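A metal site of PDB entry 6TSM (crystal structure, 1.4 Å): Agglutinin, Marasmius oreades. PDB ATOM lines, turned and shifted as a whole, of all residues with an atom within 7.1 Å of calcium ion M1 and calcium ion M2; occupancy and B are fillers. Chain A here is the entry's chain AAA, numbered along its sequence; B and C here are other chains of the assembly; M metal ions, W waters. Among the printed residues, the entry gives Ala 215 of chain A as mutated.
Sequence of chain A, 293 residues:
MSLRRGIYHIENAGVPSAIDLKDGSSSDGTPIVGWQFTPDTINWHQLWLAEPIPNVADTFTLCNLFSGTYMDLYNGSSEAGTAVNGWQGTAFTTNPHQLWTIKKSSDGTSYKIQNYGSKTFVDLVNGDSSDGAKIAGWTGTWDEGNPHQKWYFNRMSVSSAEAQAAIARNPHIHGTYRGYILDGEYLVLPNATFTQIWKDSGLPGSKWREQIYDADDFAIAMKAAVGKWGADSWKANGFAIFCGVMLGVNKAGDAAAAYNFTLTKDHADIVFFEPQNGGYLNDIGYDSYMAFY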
ATOM      1  N   ARG A 209      18.442   7.096 -14.899  1.00  0.00           N
ATOM      2  CA  ARG A 209      17.616   8.308 -14.772  1.00  0.00           C
ATOM      3  C   ARG A 209      16.178   7.949 -15.122  1.00  0.00           C
ATOM      4  O   ARG A 209      15.967   7.319 -16.174  1.00  0.00           O
ATOM      5  CB  ARG A 209      18.137   9.394 -15.697  1.00  0.00           C
ATOM      6  CG  ARG A 209      19.540   9.884 -15.324  1.00  0.00           C
ATOM      7  CD  ARG A 209      20.112  10.820 -16.375  1.00  0.00           C
ATOM      8  NE  ARG A 209      19.281  11.987 -16.549  1.00  0.00           N
ATOM      9  CZ  ARG A 209      19.382  12.846 -17.553  1.00  0.00           C
ATOM     10  NH1 ARG A 209      20.347  12.741 -18.433  1.00  0.00           N
ATOM     11  NH2 ARG A 209      18.494  13.831 -17.654  1.00  0.00           N
ATOM     12  N   GLU A 210      15.238   8.431 -14.340  1.00  0.00           N
ATOM     13  CA  GLU A 210      13.804   8.073 -14.459  1.00  0.00           C
ATOM     14  C   GLU A 210      13.321   8.384 -15.882  1.00  0.00           C
ATOM     15  O   GLU A 210      13.407   9.578 -16.280  1.00  0.00           O
ATOM     16  CB  GLU A 210      13.011   8.859 -13.405  1.00  0.00           C
ATOM     17  CG  GLU A 210      11.512   8.632 -13.448  1.00  0.00           C
ATOM     18  CD  GLU A 210      10.729   9.573 -12.514  1.00  0.00           C
ATOM     19  OE1 GLU A 210      11.373  10.228 -11.657  1.00  0.00           O
ATOM     20  OE2 GLU A 210       9.525   9.721 -12.707  1.00  0.00           O
ATOM     21  N   GLN A 211      12.898   7.341 -16.620  1.00  0.00           N
ATOM     22  CA  GLN A 211      12.329   7.360 -18.029  1.00  0.00           C
ATOM     23  C   GLN A 211      13.405   7.750 -19.075  1.00  0.00           C
ATOM     24  O   GLN A 211      13.421   7.136 -20.145  1.00  0.00           O
ATOM     25  CB  GLN A 211      11.094   8.277 -18.113  1.00  0.00           C
ATOM     26  CG  GLN A 211       9.896   7.730 -17.339  1.00  0.00           C
ATOM     27  CD  GLN A 211       8.575   8.307 -17.810  1.00  0.00           C
ATOM     28  OE1 GLN A 211       8.294   8.365 -19.001  1.00  0.00           O
ATOM     29  NE2 GLN A 211       7.765   8.733 -16.879  1.00  0.00           N
ATOM     30  N   ILE A 212      14.212   8.770 -18.809  1.00  0.00           N
ATOM     31  CA  ILE A 212      15.069   9.389 -19.866  1.00  0.00           C
ATOM     32  C   ILE A 212      16.343   8.505 -20.106  1.00  0.00           C
ATOM     33  O   ILE A 212      16.878   8.543 -21.222  1.00  0.00           O
ATOM     34  CB  ILE A 212      15.429  10.841 -19.491  1.00  0.00           C
ATOM     35  CG1 ILE A 212      16.044  11.600 -20.687  1.00  0.00           C
ATOM     36  CG2 ILE A 212      16.322  10.908 -18.268  1.00  0.00           C
ATOM     37  CD1 ILE A 212      15.106  11.796 -21.844  1.00  0.00           C
ATOM     38  N   TYR A 213      16.758   7.749 -19.123  1.00  0.00           N
ATOM     39  CA  TYR A 213      17.802   6.683 -19.366  1.00  0.00           C
ATOM     40  C   TYR A 213      17.673   5.613 -18.322  1.00  0.00           C
ATOM     41  O   TYR A 213      18.452   5.587 -17.341  1.00  0.00           O
ATOM     42  CB  TYR A 213      19.220   7.289 -19.394  1.00  0.00           C
ATOM     43  CG  TYR A 213      20.121   6.640 -20.395  1.00  0.00           C
ATOM     44  CD1 TYR A 213      19.928   6.859 -21.742  1.00  0.00           C
ATOM     45  CD2 TYR A 213      20.996   5.632 -20.022  1.00  0.00           C
ATOM     46  CE1 TYR A 213      20.701   6.209 -22.692  1.00  0.00           C
ATOM     47  CE2 TYR A 213      21.738   4.938 -20.971  1.00  0.00           C
ATOM     48  CZ  TYR A 213      21.595   5.247 -22.311  1.00  0.00           C
ATOM     49  OH  TYR A 213      22.348   4.573 -23.260  1.00  0.00           O
ATOM     50  N   ASP A 214      16.626   4.836 -18.445  1.00  0.00           N
ATOM     51  CA  ASP A 214      16.290   3.804 -17.454  1.00  0.00           C
ATOM     52  C   ASP A 214      16.524   2.414 -18.107  1.00  0.00           C
ATOM     53  O   ASP A 214      17.262   2.337 -19.090  1.00  0.00           O
ATOM     54  CB  ASP A 214      14.880   4.026 -16.908  1.00  0.00           C
ATOM     55  CG  ASP A 214      13.765   3.901 -17.933  1.00  0.00           C
ATOM     56  OD1 ASP A 214      14.027   4.137 -19.096  1.00  0.00           O
ATOM     57  OD2 ASP A 214      12.611   3.653 -17.512  1.00  0.00           O
ATOM     58  N   ALA A 215      15.966   1.362 -17.550  1.00  0.00           N
ATOM     59  CA  ALA A 215      16.383  -0.023 -17.936  1.00  0.00           C
ATOM     60  C   ALA A 215      16.251  -0.217 -19.462  1.00  0.00           C
ATOM     61  O   ALA A 215      17.148  -0.869 -20.062  1.00  0.00           O
ATOM     62  CB  ALA A 215      15.562  -1.065 -17.167  1.00  0.00           C
ATOM     63  N   ASP A 216      15.165   0.256 -20.074  1.00  0.00           N
ATOM     64  CA  ASP A 216      14.931  -0.009 -21.502  1.00  0.00           C
ATOM     65  C   ASP A 216      16.045   0.701 -22.327  1.00  0.00           C
ATOM     66  O   ASP A 216      16.497   0.121 -23.312  1.00  0.00           O
ATOM     67  CB  ASP A 216      13.513   0.409 -21.936  1.00  0.00           C
ATOM     68  CG  ASP A 216      13.084   1.754 -21.419  1.00  0.00           C
ATOM     69  OD1 ASP A 216      13.397   2.751 -22.067  1.00  0.00           O
ATOM     70  OD2 ASP A 216      12.506   1.797 -20.339  1.00  0.00           O
ATOM     71  N   ASP A 217      16.536   1.827 -21.865  1.00  0.00           N
ATOM     72  CA  ASP A 217      17.596   2.557 -22.606  1.00  0.00           C
ATOM     73  C   ASP A 217      18.900   1.756 -22.527  1.00  0.00           C
ATOM     74  O   ASP A 217      19.593   1.630 -23.566  1.00  0.00           O
ATOM     75  CB  ASP A 217      17.761   3.959 -22.075  1.00  0.00           C
ATOM     76  CG  ASP A 217      16.503   4.808 -22.258  1.00  0.00           C
ATOM     77  OD1 ASP A 217      16.220   5.171 -23.416  1.00  0.00           O
ATOM     78  OD2 ASP A 217      15.722   4.872 -21.322  1.00  0.00           O
ATOM     79  N   PHE A 218      19.228   1.231 -21.364  1.00  0.00           N
ATOM     80  CA  PHE A 218      20.473   0.421 -21.189  1.00  0.00           C
ATOM     81  C   PHE A 218      20.420  -0.828 -22.089  1.00  0.00           C
ATOM     82  O   PHE A 218      21.381  -1.126 -22.760  1.00  0.00           O
ATOM     83  CB  PHE A 218      20.682   0.041 -19.735  1.00  0.00           C
ATOM     84  CG  PHE A 218      21.255   1.124 -18.868  1.00  0.00           C
ATOM     85  CD1 PHE A 218      20.438   2.077 -18.293  1.00  0.00           C
ATOM     86  CD2 PHE A 218      22.616   1.166 -18.596  1.00  0.00           C
ATOM     87  CE1 PHE A 218      20.945   3.023 -17.412  1.00  0.00           C
ATOM     88  CE2 PHE A 218      23.140   2.137 -17.756  1.00  0.00           C
ATOM     89  CZ  PHE A 218      22.295   3.060 -17.169  1.00  0.00           C
ATOM     90  N   VAL B   2       5.378  -0.522 -15.063  1.00  0.00           N
ATOM     91  CA  VAL B   2       6.117   0.145 -16.180  1.00  0.00           C
ATOM     92  C   VAL B   2       7.569  -0.378 -16.190  1.00  0.00           C
ATOM     93  O   VAL B   2       8.084  -0.721 -15.101  1.00  0.00           O
ATOM     94  CB  VAL B   2       6.059   1.680 -16.061  1.00  0.00           C
ATOM     95  CG1 VAL B   2       4.644   2.201 -16.214  1.00  0.00           C
ATOM     96  CG2 VAL B   2       6.691   2.182 -14.763  1.00  0.00           C
ATOM     97  N   VAL B   3       8.126  -0.570 -17.390  1.00  0.00           N
ATOM     98  CA  VAL B   3       9.528  -1.055 -17.587  1.00  0.00           C
ATOM     99  C   VAL B   3      10.489   0.012 -17.073  1.00  0.00           C
ATOM    100  O   VAL B   3      10.517   1.108 -17.657  1.00  0.00           O
ATOM    101  CB  VAL B   3       9.809  -1.369 -19.067  1.00  0.00           C
ATOM    102  CG1 VAL B   3      11.281  -1.653 -19.318  1.00  0.00           C
ATOM    103  CG2 VAL B   3       8.950  -2.538 -19.560  1.00  0.00           C
ATOM    104  N   ARG B   4      11.185  -0.277 -15.967  1.00  0.00           N
ATOM    105  CA  ARG B   4      11.942   0.751 -15.176  1.00  0.00           C
ATOM    106  C   ARG B   4      13.349   0.240 -14.892  1.00  0.00           C
ATOM    107  O   ARG B   4      14.295   1.023 -14.951  1.00  0.00           O
ATOM    108  CB  ARG B   4      11.221   1.045 -13.862  1.00  0.00           C
ATOM    109  CG  ARG B   4      10.058   2.010 -14.001  1.00  0.00           C
ATOM    110  CD  ARG B   4       9.518   2.453 -12.650  1.00  0.00           C
ATOM    111  NE  ARG B   4      10.448   3.333 -11.934  1.00  0.00           N
ATOM    112  CZ  ARG B   4      11.161   2.975 -10.871  1.00  0.00           C
ATOM    113  NH1 ARG B   4      11.080   1.745 -10.383  1.00  0.00           N
ATOM    114  NH2 ARG B   4      11.949   3.857 -10.284  1.00  0.00           N
ATOM    115  OXT ARG B   4      13.565  -0.985 -14.529  1.00  0.00           O
ATOM    116  N   ILE C 181       5.042  -1.047 -24.551  1.00  0.00           N
ATOM    117  CA  ILE C 181       5.298   0.320 -24.058  1.00  0.00           C
ATOM    118  C   ILE C 181       6.470   0.281 -23.049  1.00  0.00           C
ATOM    119  O   ILE C 181       6.464  -0.594 -22.173  1.00  0.00           O
ATOM    120  CB  ILE C 181       4.025   0.897 -23.419  1.00  0.00           C
ATOM    121  CG1 ILE C 181       2.926   1.079 -24.474  1.00  0.00           C
ATOM    122  CG2 ILE C 181       4.324   2.170 -22.690  1.00  0.00           C
ATOM    123  CD1 ILE C 181       1.578   1.375 -23.901  1.00  0.00           C
ATOM    124  N   LEU C 182       7.370   1.262 -23.132  1.00  0.00           N
ATOM    125  CA  LEU C 182       8.623   1.239 -22.330  1.00  0.00           C
ATOM    126  C   LEU C 182       8.610   2.366 -21.276  1.00  0.00           C
ATOM    127  O   LEU C 182       9.352   2.219 -20.243  1.00  0.00           O
ATOM    128  CB  LEU C 182       9.819   1.379 -23.267  1.00  0.00           C
ATOM    129  CG  LEU C 182       9.956   0.282 -24.311  1.00  0.00           C
ATOM    130  CD1 LEU C 182      11.135   0.564 -25.226  1.00  0.00           C
ATOM    131  CD2 LEU C 182      10.114  -1.080 -23.663  1.00  0.00           C
ATOM    132  N   ASP C 183       7.928   3.492 -21.562  1.00  0.00           N
ATOM    133  CA  ASP C 183       7.984   4.711 -20.714  1.00  0.00           C
ATOM    134  C   ASP C 183       6.572   5.327 -20.635  1.00  0.00           C
ATOM    135  O   ASP C 183       5.625   4.670 -21.107  1.00  0.00           O
ATOM    136  CB  ASP C 183       9.012   5.717 -21.259  1.00  0.00           C
ATOM    137  CG  ASP C 183      10.471   5.207 -21.230  1.00  0.00           C
ATOM    138  OD1 ASP C 183      10.948   4.865 -20.157  1.00  0.00           O
ATOM    139  OD2 ASP C 183      11.112   5.215 -22.294  1.00  0.00           O
ATOM    140  N   GLY C 184       6.438   6.435 -19.943  1.00  0.00           N
ATOM    141  CA  GLY C 184       5.116   6.984 -19.561  1.00  0.00           C
ATOM    142  C   GLY C 184       4.766   8.256 -20.355  1.00  0.00           C
ATOM    143  O   GLY C 184       3.571   8.526 -20.508  1.00  0.00           O
ATOM    144  N   TYR C 186       6.351  11.226 -23.225  1.00  0.00           N
ATOM    145  CA  TYR C 186       7.353  11.335 -24.327  1.00  0.00           C
ATOM    146  C   TYR C 186       7.344  12.751 -24.896  1.00  0.00           C
ATOM    147  O   TYR C 186       6.313  13.162 -25.462  1.00  0.00           O
ATOM    148  CB  TYR C 186       7.045  10.350 -25.425  1.00  0.00           C
ATOM    149  CG  TYR C 186       7.058   8.910 -25.007  1.00  0.00           C
ATOM    150  CD1 TYR C 186       5.911   8.284 -24.540  1.00  0.00           C
ATOM    151  CD2 TYR C 186       8.192   8.144 -25.145  1.00  0.00           C
ATOM    152  CE1 TYR C 186       5.885   6.923 -24.288  1.00  0.00           C
ATOM    153  CE2 TYR C 186       8.199   6.791 -24.856  1.00  0.00           C
ATOM    154  CZ  TYR C 186       7.041   6.182 -24.407  1.00  0.00           C
ATOM    155  OH  TYR C 186       7.039   4.838 -24.158  1.00  0.00           O
ATOM    156  N   LYS C 223      16.835   4.025 -32.665  1.00  0.00           N
ATOM    157  CA  LYS C 223      16.211   4.168 -31.350  1.00  0.00           C
ATOM    158  C   LYS C 223      17.301   4.429 -30.281  1.00  0.00           C
ATOM    159  O   LYS C 223      17.091   5.265 -29.434  1.00  0.00           O
ATOM    160  CB  LYS C 223      15.401   2.930 -30.974  1.00  0.00           C
ATOM    161  CG  LYS C 223      14.728   3.026 -29.615  1.00  0.00           C
ATOM    162  CD  LYS C 223      13.360   2.402 -29.541  1.00  0.00           C
ATOM    163  CE  LYS C 223      12.719   2.541 -28.165  1.00  0.00           C
ATOM    164  NZ  LYS C 223      12.619   3.958 -27.723  1.00  0.00           N
ATOM    165  N   PHE C 239      10.724  11.799 -18.052  1.00  0.00           N
ATOM    166  CA  PHE C 239      10.166  11.750 -19.412  1.00  0.00           C
ATOM    167  C   PHE C 239      11.140  11.013 -20.340  1.00  0.00           C
ATOM    168  O   PHE C 239      12.317  10.836 -19.944  1.00  0.00           O
ATOM    169  CB  PHE C 239       9.896  13.152 -19.930  1.00  0.00           C
ATOM    170  CG  PHE C 239      11.153  13.922 -20.235  1.00  0.00           C
ATOM    171  CD1 PHE C 239      11.942  14.445 -19.210  1.00  0.00           C
ATOM    172  CD2 PHE C 239      11.579  14.092 -21.532  1.00  0.00           C
ATOM    173  CE1 PHE C 239      13.152  15.066 -19.502  1.00  0.00           C
ATOM    174  CE2 PHE C 239      12.774  14.738 -21.813  1.00  0.00           C
ATOM    175  CZ  PHE C 239      13.549  15.205 -20.797  1.00  0.00           C
ATOM    176  N   ALA C 240      10.665  10.615 -21.509  1.00  0.00           N
ATOM    177  CA  ALA C 240      11.501  10.022 -22.564  1.00  0.00           C
ATOM    178  C   ALA C 240      11.291  10.774 -23.875  1.00  0.00           C
ATOM    179  O   ALA C 240      10.465  11.709 -23.891  1.00  0.00           O
ATOM    180  CB  ALA C 240      11.161   8.546 -22.720  1.00  0.00           C
ATOM    181  N   ILE C 241      12.084  10.460 -24.874  1.00  0.00           N
ATOM    182  CA  ILE C 241      11.927  11.011 -26.242  1.00  0.00           C
ATOM    183  C   ILE C 241      11.161   9.992 -27.072  1.00  0.00           C
ATOM    184  O   ILE C 241      11.532   8.802 -27.042  1.00  0.00           O
ATOM    185  CB  ILE C 241      13.308  11.345 -26.871  1.00  0.00           C
ATOM    186  CG1 ILE C 241      14.233  12.076 -25.895  1.00  0.00           C
ATOM    187  CG2 ILE C 241      13.120  12.120 -28.153  1.00  0.00           C
ATOM    188  CD1 ILE C 241      13.665  13.329 -25.307  1.00  0.00           C
ATOM    189  N   TYR C 293       8.271   1.055 -27.982  1.00  0.00           N
ATOM    190  CA  TYR C 293       8.399   2.534 -27.929  1.00  0.00           C
ATOM    191  C   TYR C 293       8.266   2.982 -26.510  1.00  0.00           C
ATOM    192  O   TYR C 293       8.812   3.994 -26.133  1.00  0.00           O
ATOM    193  CB  TYR C 293       7.347   3.200 -28.822  1.00  0.00           C
ATOM    194  CG  TYR C 293       5.920   2.830 -28.480  1.00  0.00           C
ATOM    195  CD1 TYR C 293       5.317   1.720 -29.034  1.00  0.00           C
ATOM    196  CD2 TYR C 293       5.138   3.662 -27.688  1.00  0.00           C
ATOM    197  CE1 TYR C 293       3.981   1.402 -28.779  1.00  0.00           C
ATOM    198  CE2 TYR C 293       3.815   3.348 -27.384  1.00  0.00           C
ATOM    199  CZ  TYR C 293       3.222   2.235 -27.968  1.00  0.00           C
ATOM    200  OH  TYR C 293       1.902   1.914 -27.695  1.00  0.00           O
ATOM    201  OXT TYR C 293       7.595   2.304 -25.690  1.00  0.00           O
HETATM  202 CA    CA M   1      10.998   2.780 -18.875  1.00  0.00          CA
HETATM  203 CA    CA M   2      13.321   4.998 -21.169  1.00  0.00          CA
HETATM  204  O   HOH W   1       9.379   3.912 -17.311  1.00  0.00           O
HETATM  205  O   HOH W   2      13.791   6.005 -23.304  1.00  0.00           O
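Of the 23 residues printed, 5 come within 4 Å of calcium ion M2. The nearest printed residue that does not touch calcium ion M2 is Ala 240 of chain C (4.4 Å).
Calcium ion M1 is bound by O of Val 3 of chain B (2.1 Å), O of Leu 182 of chain C (2.2 Å), OD2 of Asp 214 (2.3 Å), OD2 of Asp 216 (2.3 Å), OD1 of Asp 183 of chain C (2.4 Å) and water W1 (2.5 Å).
N of Leu 182 of chain C lies within hydrogen-bond range of OXT of Tyr 293 of chain C (2.8 Å). The side-chain amide oxygen (OE1) of Gln 211 is in hydrogen-bond range of the backbone NH (N) of Gly 184 of chain C. The backbone carbonyl oxygen (O) of Arg 209 lies within hydrogen-bond range of the backbone NH (N) of Asp 214 (3.4 Å). The backbone NH (N) of Asp 183 of chain C sits at hydrogen-bond distance from the side-chain hydroxyl (OH) of Tyr 186 of chain C, at 3.1 Å.
Calcium ion M2 is bound by the side-chain carboxylate (OD1) of Asp 214 (2.4 Å), the backbone carbonyl oxygen (O) of Gln 211 (2.4 Å), water W2 (2.4 Å), the side-chain carboxylate (OD2) of Asp 217 (2.4 Å), the side-chain carboxylate (OD1) of Asp 216 (2.4 Å), the side-chain carboxylate (OD2) of Asp 183 of chain C (2.5 Å) and the side-chain carboxylate (OD1) of Asp 183 of chain C (2.6 Å).
Of the 23 residues printed, 5 come within 4 Å of calcium ion M1. Along chain A the residues within 4 Å of calcium ion M1 span positions 214 to 216. The nearest printed residue that does not touch calcium ion M1 is Arg 4 of chain B (4.2 Å).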
